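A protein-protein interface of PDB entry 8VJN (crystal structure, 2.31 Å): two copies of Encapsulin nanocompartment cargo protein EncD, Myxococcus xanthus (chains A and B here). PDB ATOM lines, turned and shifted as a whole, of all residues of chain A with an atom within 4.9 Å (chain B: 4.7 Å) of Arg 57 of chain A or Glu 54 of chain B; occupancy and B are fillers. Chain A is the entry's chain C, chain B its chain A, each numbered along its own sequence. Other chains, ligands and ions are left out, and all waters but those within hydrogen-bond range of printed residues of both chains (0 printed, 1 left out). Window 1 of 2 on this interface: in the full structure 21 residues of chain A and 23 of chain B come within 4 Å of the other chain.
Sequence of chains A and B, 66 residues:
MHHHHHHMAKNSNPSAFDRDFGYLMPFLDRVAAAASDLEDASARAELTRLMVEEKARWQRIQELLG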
ATOM      1  N   GLU A  53      17.584  -0.051  -6.344  1.00  0.00           N
ATOM      2  CA  GLU A  53      16.658  -0.573  -5.334  1.00  0.00           C
ATOM      3  C   GLU A  53      16.514  -2.086  -5.428  1.00  0.00           C
ATOM      4  O   GLU A  53      16.313  -2.777  -4.413  1.00  0.00           O
ATOM      5  CB  GLU A  53      15.279   0.051  -5.493  1.00  0.00           C
ATOM      6  CG  GLU A  53      15.215   1.559  -5.361  1.00  0.00           C
ATOM      7  CD  GLU A  53      13.817   2.084  -5.671  1.00  0.00           C
ATOM      8  OE1 GLU A  53      12.963   1.275  -6.123  1.00  0.00           O
ATOM      9  OE2 GLU A  53      13.570   3.296  -5.453  1.00  0.00           O
ATOM     10  N   GLU A  54      16.619  -2.608  -6.643  1.00  0.00           N
ATOM     11  CA  GLU A  54      16.412  -4.030  -6.849  1.00  0.00           C
ATOM     12  C   GLU A  54      17.537  -4.828  -6.235  1.00  0.00           C
ATOM     13  O   GLU A  54      17.302  -5.934  -5.740  1.00  0.00           O
ATOM     14  CB  GLU A  54      16.320  -4.365  -8.335  1.00  0.00           C
ATOM     15  CG  GLU A  54      14.944  -4.095  -8.930  1.00  0.00           C
ATOM     16  CD  GLU A  54      13.834  -4.775  -8.163  1.00  0.00           C
ATOM     17  OE1 GLU A  54      14.004  -5.965  -7.845  1.00  0.00           O
ATOM     18  OE2 GLU A  54      12.804  -4.125  -7.874  1.00  0.00           O
ATOM     19  N   LYS A  55      18.763  -4.284  -6.234  1.00  0.00           N
ATOM     20  CA  LYS A  55      19.888  -5.013  -5.634  1.00  0.00           C
ATOM     21  C   LYS A  55      19.693  -5.225  -4.131  1.00  0.00           C
ATOM     22  O   LYS A  55      19.868  -6.350  -3.615  1.00  0.00           O
ATOM     23  CB  LYS A  55      21.192  -4.270  -5.892  1.00  0.00           C
ATOM     24  CG  LYS A  55      21.647  -4.259  -7.340  1.00  0.00           C
ATOM     25  CD  LYS A  55      21.528  -5.629  -8.021  1.00  0.00           C
ATOM     26  CE  LYS A  55      22.385  -5.671  -9.269  1.00  0.00           C
ATOM     27  NZ  LYS A  55      21.740  -4.940 -10.391  1.00  0.00           N
ATOM     28  N   ALA A  56      19.308  -4.170  -3.417  1.00  0.00           N
ATOM     29  CA  ALA A  56      19.031  -4.305  -1.984  1.00  0.00           C
ATOM     30  C   ALA A  56      17.847  -5.231  -1.728  1.00  0.00           C
ATOM     31  O   ALA A  56      17.881  -6.060  -0.801  1.00  0.00           O
ATOM     32  CB  ALA A  56      18.753  -2.936  -1.344  1.00  0.00           C
ATOM     33  N   ARG A  57      16.784  -5.089  -2.528  1.00  0.00           N
ATOM     34  CA  ARG A  57      15.632  -5.966  -2.397  1.00  0.00           C
ATOM     35  C   ARG A  57      16.013  -7.428  -2.571  1.00  0.00           C
ATOM     36  O   ARG A  57      15.628  -8.271  -1.760  1.00  0.00           O
ATOM     37  CB  ARG A  57      14.561  -5.565  -3.399  1.00  0.00           C
ATOM     38  CG  ARG A  57      13.746  -4.413  -2.919  1.00  0.00           C
ATOM     39  CD  ARG A  57      12.906  -3.836  -3.991  1.00  0.00           C
ATOM     40  NE  ARG A  57      12.078  -2.777  -3.443  1.00  0.00           N
ATOM     41  CZ  ARG A  57      10.797  -2.906  -3.147  1.00  0.00           C
ATOM     42  NH1 ARG A  57      10.145  -4.033  -3.393  1.00  0.00           N
ATOM     43  NH2 ARG A  57      10.156  -1.875  -2.594  1.00  0.00           N
ATOM     44  N   TRP A  58      16.796  -7.750  -3.599  1.00  0.00           N
ATOM     45  CA  TRP A  58      17.126  -9.154  -3.831  1.00  0.00           C
ATOM     46  C   TRP A  58      18.073  -9.713  -2.773  1.00  0.00           C
ATOM     47  O   TRP A  58      17.958 -10.896  -2.414  1.00  0.00           O
ATOM     48  CB  TRP A  58      17.674  -9.322  -5.241  1.00  0.00           C
ATOM     49  CG  TRP A  58      16.501  -9.353  -6.101  1.00  0.00           C
ATOM     50  CD1 TRP A  58      16.048  -8.365  -6.890  1.00  0.00           C
ATOM     51  CD2 TRP A  58      15.532 -10.409  -6.170  1.00  0.00           C
ATOM     52  NE1 TRP A  58      14.863  -8.732  -7.476  1.00  0.00           N
ATOM     53  CE2 TRP A  58      14.527  -9.990  -7.057  1.00  0.00           C
ATOM     54  CE3 TRP A  58      15.431 -11.677  -5.576  1.00  0.00           C
ATOM     55  CZ2 TRP A  58      13.429 -10.794  -7.382  1.00  0.00           C
ATOM     56  CZ3 TRP A  58      14.354 -12.478  -5.900  1.00  0.00           C
ATOM     57  CH2 TRP A  58      13.361 -12.037  -6.797  1.00  0.00           C
ATOM     58  N   GLN A  59      18.963  -8.873  -2.230  1.00  0.00           N
ATOM     59  CA  GLN A  59      19.736  -9.257  -1.045  1.00  0.00           C
ATOM     60  C   GLN A  59      18.819  -9.625   0.127  1.00  0.00           C
ATOM     61  O   GLN A  59      18.999 -10.670   0.769  1.00  0.00           O
ATOM     62  CB  GLN A  59      20.689  -8.116  -0.679  1.00  0.00           C
ATOM     63  CG  GLN A  59      22.111  -8.528  -0.277  1.00  0.00           C
ATOM     64  CD  GLN A  59      22.213  -9.442   0.957  1.00  0.00           C
ATOM     65  OE1 GLN A  59      21.312  -9.499   1.797  1.00  0.00           O
ATOM     66  NE2 GLN A  59      23.318 -10.185   1.044  1.00  0.00           N
ATOM     67  N   ARG A  60      17.792  -8.805   0.382  1.00  0.00           N
ATOM     68  CA  ARG A  60      16.857  -9.107   1.476  1.00  0.00           C
ATOM     69  C   ARG A  60      16.010 -10.349   1.185  1.00  0.00           C
ATOM     70  O   ARG A  60      15.719 -11.146   2.089  1.00  0.00           O
ATOM     71  CB  ARG A  60      15.959  -7.894   1.738  1.00  0.00           C
ATOM     72  CG  ARG A  60      14.947  -8.067   2.857  1.00  0.00           C
ATOM     73  CD  ARG A  60      15.580  -8.596   4.167  1.00  0.00           C
ATOM     74  NE  ARG A  60      14.793  -8.247   5.350  1.00  0.00           N
ATOM     75  CZ  ARG A  60      14.782  -8.937   6.487  1.00  0.00           C
ATOM     76  NH1 ARG A  60      15.533 -10.016   6.651  1.00  0.00           N
ATOM     77  NH2 ARG A  60      14.006  -8.526   7.489  1.00  0.00           N
ATOM     78  N   ILE A  61      15.597 -10.517  -0.068  1.00  0.00           N
ATOM     79  CA  ILE A  61      14.741 -11.635  -0.438  1.00  0.00           C
ATOM     80  C   ILE A  61      15.474 -12.943  -0.232  1.00  0.00           C
ATOM     81  O   ILE A  61      14.931 -13.891   0.346  1.00  0.00           O
ATOM     82  CB  ILE A  61      14.272 -11.488  -1.892  1.00  0.00           C
ATOM     83  CG1 ILE A  61      13.198 -10.412  -1.979  1.00  0.00           C
ATOM     84  CG2 ILE A  61      13.755 -12.817  -2.405  1.00  0.00           C
ATOM     85  CD1 ILE A  61      13.189  -9.672  -3.281  1.00  0.00           C
ATOM     86  N   LEU B  28       9.248 -15.269  -9.936  1.00  0.00           N
ATOM     87  CA  LEU B  28       8.591 -14.434  -8.919  1.00  0.00           C
ATOM     88  C   LEU B  28       7.386 -15.137  -8.299  1.00  0.00           C
ATOM     89  O   LEU B  28       7.178 -15.063  -7.079  1.00  0.00           O
ATOM     90  CB  LEU B  28       8.165 -13.096  -9.525  1.00  0.00           C
ATOM     91  CG  LEU B  28       9.393 -12.292  -9.909  1.00  0.00           C
ATOM     92  CD1 LEU B  28       9.028 -11.079 -10.735  1.00  0.00           C
ATOM     93  CD2 LEU B  28      10.119 -11.910  -8.628  1.00  0.00           C
ATOM     94  N   LEU B  50       7.052  -8.316  -0.303  1.00  0.00           N
ATOM     95  CA  LEU B  50       8.149  -8.140  -1.250  1.00  0.00           C
ATOM     96  C   LEU B  50       7.823  -8.727  -2.616  1.00  0.00           C
ATOM     97  O   LEU B  50       8.081  -8.093  -3.638  1.00  0.00           O
ATOM     98  CB  LEU B  50       9.431  -8.766  -0.692  1.00  0.00           C
ATOM     99  CG  LEU B  50      10.306  -7.745   0.032  1.00  0.00           C
ATOM    100  CD1 LEU B  50      11.379  -8.435   0.857  1.00  0.00           C
ATOM    101  CD2 LEU B  50      10.916  -6.781  -0.979  1.00  0.00           C
ATOM    102  N   MET B  51       7.255  -9.929  -2.666  1.00  0.00           N
ATOM    103  CA  MET B  51       6.996 -10.536  -3.970  1.00  0.00           C
ATOM    104  C   MET B  51       5.911  -9.815  -4.741  1.00  0.00           C
ATOM    105  O   MET B  51       6.036  -9.681  -5.970  1.00  0.00           O
ATOM    106  CB  MET B  51       6.645 -12.005  -3.828  1.00  0.00           C
ATOM    107  CG  MET B  51       7.869 -12.913  -3.826  1.00  0.00           C
ATOM    108  SD  MET B  51       9.259 -12.368  -4.869  1.00  0.00           S
ATOM    109  CE  MET B  51      10.258 -11.678  -3.604  1.00  0.00           C
ATOM    110  N   VAL B  52       4.854  -9.355  -4.043  1.00  0.00           N
ATOM    111  CA  VAL B  52       3.844  -8.487  -4.658  1.00  0.00           C
ATOM    112  C   VAL B  52       4.496  -7.283  -5.339  1.00  0.00           C
ATOM    113  O   VAL B  52       4.249  -6.998  -6.532  1.00  0.00           O
ATOM    114  CB  VAL B  52       2.822  -8.035  -3.597  1.00  0.00           C
ATOM    115  CG1 VAL B  52       1.701  -7.266  -4.233  1.00  0.00           C
ATOM    116  CG2 VAL B  52       2.212  -9.231  -2.920  1.00  0.00           C
ATOM    117  N   GLU B  53       5.353  -6.560  -4.588  1.00  0.00           N
ATOM    118  CA  GLU B  53       5.997  -5.378  -5.160  1.00  0.00           C
ATOM    119  C   GLU B  53       6.917  -5.749  -6.306  1.00  0.00           C
ATOM    120  O   GLU B  53       6.984  -5.032  -7.306  1.00  0.00           O
ATOM    121  CB  GLU B  53       6.799  -4.592  -4.120  1.00  0.00           C
ATOM    122  CG  GLU B  53       6.017  -3.965  -3.000  1.00  0.00           C
ATOM    123  CD  GLU B  53       6.859  -3.833  -1.742  1.00  0.00           C
ATOM    124  OE1 GLU B  53       7.396  -4.849  -1.275  1.00  0.00           O
ATOM    125  OE2 GLU B  53       7.029  -2.706  -1.235  1.00  0.00           O
ATOM    126  N   GLU B  54       7.655  -6.846  -6.153  1.00  0.00           N
ATOM    127  CA  GLU B  54       8.555  -7.326  -7.192  1.00  0.00           C
ATOM    128  C   GLU B  54       7.815  -7.542  -8.495  1.00  0.00           C
ATOM    129  O   GLU B  54       8.325  -7.204  -9.571  1.00  0.00           O
ATOM    130  CB  GLU B  54       9.188  -8.633  -6.742  1.00  0.00           C
ATOM    131  CG  GLU B  54      10.359  -8.468  -5.827  1.00  0.00           C
ATOM    132  CD  GLU B  54      11.253  -7.360  -6.275  1.00  0.00           C
ATOM    133  OE1 GLU B  54      11.803  -7.502  -7.381  1.00  0.00           O
ATOM    134  OE2 GLU B  54      11.412  -6.364  -5.531  1.00  0.00           O
ATOM    135  N   LYS B  55       6.598  -8.080  -8.404  1.00  0.00           N
ATOM    136  CA  LYS B  55       5.788  -8.298  -9.594  1.00  0.00           C
ATOM    137  C   LYS B  55       5.436  -6.981 -10.263  1.00  0.00           C
ATOM    138  O   LYS B  55       5.647  -6.806 -11.482  1.00  0.00           O
ATOM    139  CB  LYS B  55       4.542  -9.092  -9.204  1.00  0.00           C
ATOM    140  CG  LYS B  55       4.737 -10.613  -9.292  1.00  0.00           C
ATOM    141  CD  LYS B  55       3.859 -11.373  -8.305  1.00  0.00           C
ATOM    142  CE  LYS B  55       4.627 -12.523  -7.636  1.00  0.00           C
ATOM    143  NZ  LYS B  55       3.714 -13.664  -7.261  1.00  0.00           N
ATOM    144  N   ALA B  56       4.934  -6.016  -9.471  1.00  0.00           N
ATOM    145  CA  ALA B  56       4.566  -4.718 -10.042  1.00  0.00           C
ATOM    146  C   ALA B  56       5.781  -4.020 -10.648  1.00  0.00           C
ATOM    147  O   ALA B  56       5.730  -3.496 -11.778  1.00  0.00           O
ATOM    148  CB  ALA B  56       3.919  -3.833  -8.974  1.00  0.00           C
ATOM    149  N   ARG B  57       6.895  -4.031  -9.903  1.00  0.00           N
ATOM    150  CA  ARG B  57       8.106  -3.352 -10.328  1.00  0.00           C
ATOM    151  C   ARG B  57       8.694  -3.977 -11.585  1.00  0.00           C
ATOM    152  O   ARG B  57       9.101  -3.249 -12.497  1.00  0.00           O
ATOM    153  CB  ARG B  57       9.108  -3.366  -9.190  1.00  0.00           C
ATOM    154  CG  ARG B  57       8.693  -2.376  -8.103  1.00  0.00           C
ATOM    155  CD  ARG B  57       9.151  -2.805  -6.749  1.00  0.00           C
ATOM    156  NE  ARG B  57      10.594  -2.717  -6.716  1.00  0.00           N
ATOM    157  CZ  ARG B  57      11.240  -1.604  -6.425  1.00  0.00           C
ATOM    158  NH1 ARG B  57      10.589  -0.505  -6.079  1.00  0.00           N
ATOM    159  NH2 ARG B  57      12.569  -1.592  -6.489  1.00  0.00           N
ATOM    160  N   TRP B  58       8.739  -5.307 -11.679  1.00  0.00           N
ATOM    161  CA  TRP B  58       9.297  -5.869 -12.911  1.00  0.00           C
ATOM    162  C   TRP B  58       8.379  -5.675 -14.112  1.00  0.00           C
ATOM    163  O   TRP B  58       8.895  -5.564 -15.231  1.00  0.00           O
ATOM    164  CB  TRP B  58       9.663  -7.341 -12.734  1.00  0.00           C
ATOM    165  CG  TRP B  58      10.978  -7.386 -12.044  1.00  0.00           C
ATOM    166  CD1 TRP B  58      11.196  -7.600 -10.715  1.00  0.00           C
ATOM    167  CD2 TRP B  58      12.249  -7.083 -12.620  1.00  0.00           C
ATOM    168  NE1 TRP B  58      12.534  -7.483 -10.434  1.00  0.00           N
ATOM    169  CE2 TRP B  58      13.204  -7.173 -11.594  1.00  0.00           C
ATOM    170  CE3 TRP B  58      12.681  -6.774 -13.918  1.00  0.00           C
ATOM    171  CZ2 TRP B  58      14.560  -6.961 -11.815  1.00  0.00           C
ATOM    172  CZ3 TRP B  58      14.013  -6.563 -14.137  1.00  0.00           C
ATOM    173  CH2 TRP B  58      14.948  -6.660 -13.088  1.00  0.00           C
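The guanidinium group (NH1) of Arg 57 of chain A lies within salt-bridge range of the side-chain carboxylate (OE2) of Glu 54 of chain B. The side-chain carboxylate of Glu 54 of chain B lies close to the side-chain carboxylate of Glu 54 of chain A (2.7 Å). The side-chain carboxylate (OE1) of Glu 54 of chain A sits at hydrogen-bond distance from the indole nitrogen (NE1) of Trp 58 of chain B, 3.3 Å away. The side-chain carboxylate (OE1) of Glu 54 of chain B lies within hydrogen-bond range of the indole nitrogen (NE1) of Trp 58 of chain A (3.3 Å). NH2 of Arg 57 of chain B is in salt-bridge range of OE1 of Glu 53 of chain A, at 2.9 Å. The guanidinium group (NE) of Arg 57 of chain A lies close to the guanidinium group (NH2) of Arg 57 of chain B, at 3.3 Å. The guanidinium group of Arg 57 of chain B lies within salt-bridge range of the side-chain carboxylate of Glu 54 of chain A (2.9 Å). The guanidinium group (NH2) of Arg 57 of chain A lies within salt-bridge range of the side-chain carboxylate (OE2) of Glu 53 of chain B (3.5 Å).
The side-chain carboxylate of Glu 54 of chain A is in hydrogen-bond range of the indole nitrogen of Trp 58 of chain A (2.9 Å). NE1 of Trp 58 of chain B sits at hydrogen-bond distance from OE1 of Glu 54 of chain B. The guanidinium group of Arg 57 of chain B is in salt-bridge range of the side-chain carboxylate of Glu 54 of chain B (3.9 Å).
Among the printed residues, pairs that only touch across the chains: Arg 57 of chain A with Leu 50 of chain B, Trp 58 of chain A with Leu 28 of chain B, Trp 58 of chain A with Trp 58 of chain B, Ile 61 of chain A with Leu 50 of chain B, Ile 61 of chain A with Met 51 of chain B and Ile 61 of chain A with Glu 54 of chain B.
Of chain B, only Leu 50, Glu 53, Glu 54 and Arg 57 come within 4 Å of Arg 57 of chain A. Of the printed residues of chain A, Glu 54 of chain B touches Glu 54, Arg 57, Trp 58 and Ile 61. Printed residues of chain A within 4 Å of Met 51 of chain B: Ile 61 (3.6 Å). Of the printed residues of chain B, Trp 58 of chain A touches Leu 28, Glu 54 and Trp 58. Lys 55 of chain B touches none of the printed residues of chain A. The nearest printed residue of chain B that does not touch Arg 57 of chain A is Met 51 of chain B (6.6 Å). The nearest printed residue of chain B that does not touch Trp 58 of chain A is Met 51 of chain B (4.5 Å).
Of the 9 printed residues of chain A, 5 touch a printed residue of chain B. Hydrophobic or aromatic side chains of chain A that line the printed part of chain B: Trp 58 and Ile 61. Of the 10 printed residues of chain B, 7 touch a printed residue of chain A. Hydrophobic or aromatic side chains of chain B that line the printed part of chain A: Leu 28, Leu 50, Met 51 and Trp 58. Among the printed residues, 14 pairs touch across the chains.
Glu 53 of chain A touches Arg 57 of chain B, and with the chains exchanged Arg 57 of chain A touches Glu 53 of chain B. Glu 54 of chain A touches its own counterpart, Glu 54 of chain B. Glu 54 of chain A touches Arg 57 of chain B, and with the chains exchanged Arg 57 of chain A touches Glu 54 of chain B. Glu 54 of chain A touches Trp 58 of chain B, and with the chains exchanged Trp 58 of chain A touches Glu 54 of chain B. Of the 14 pairs that touch across the chains among the printed residues, 9 have their exchanged pair printed and touching as well.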
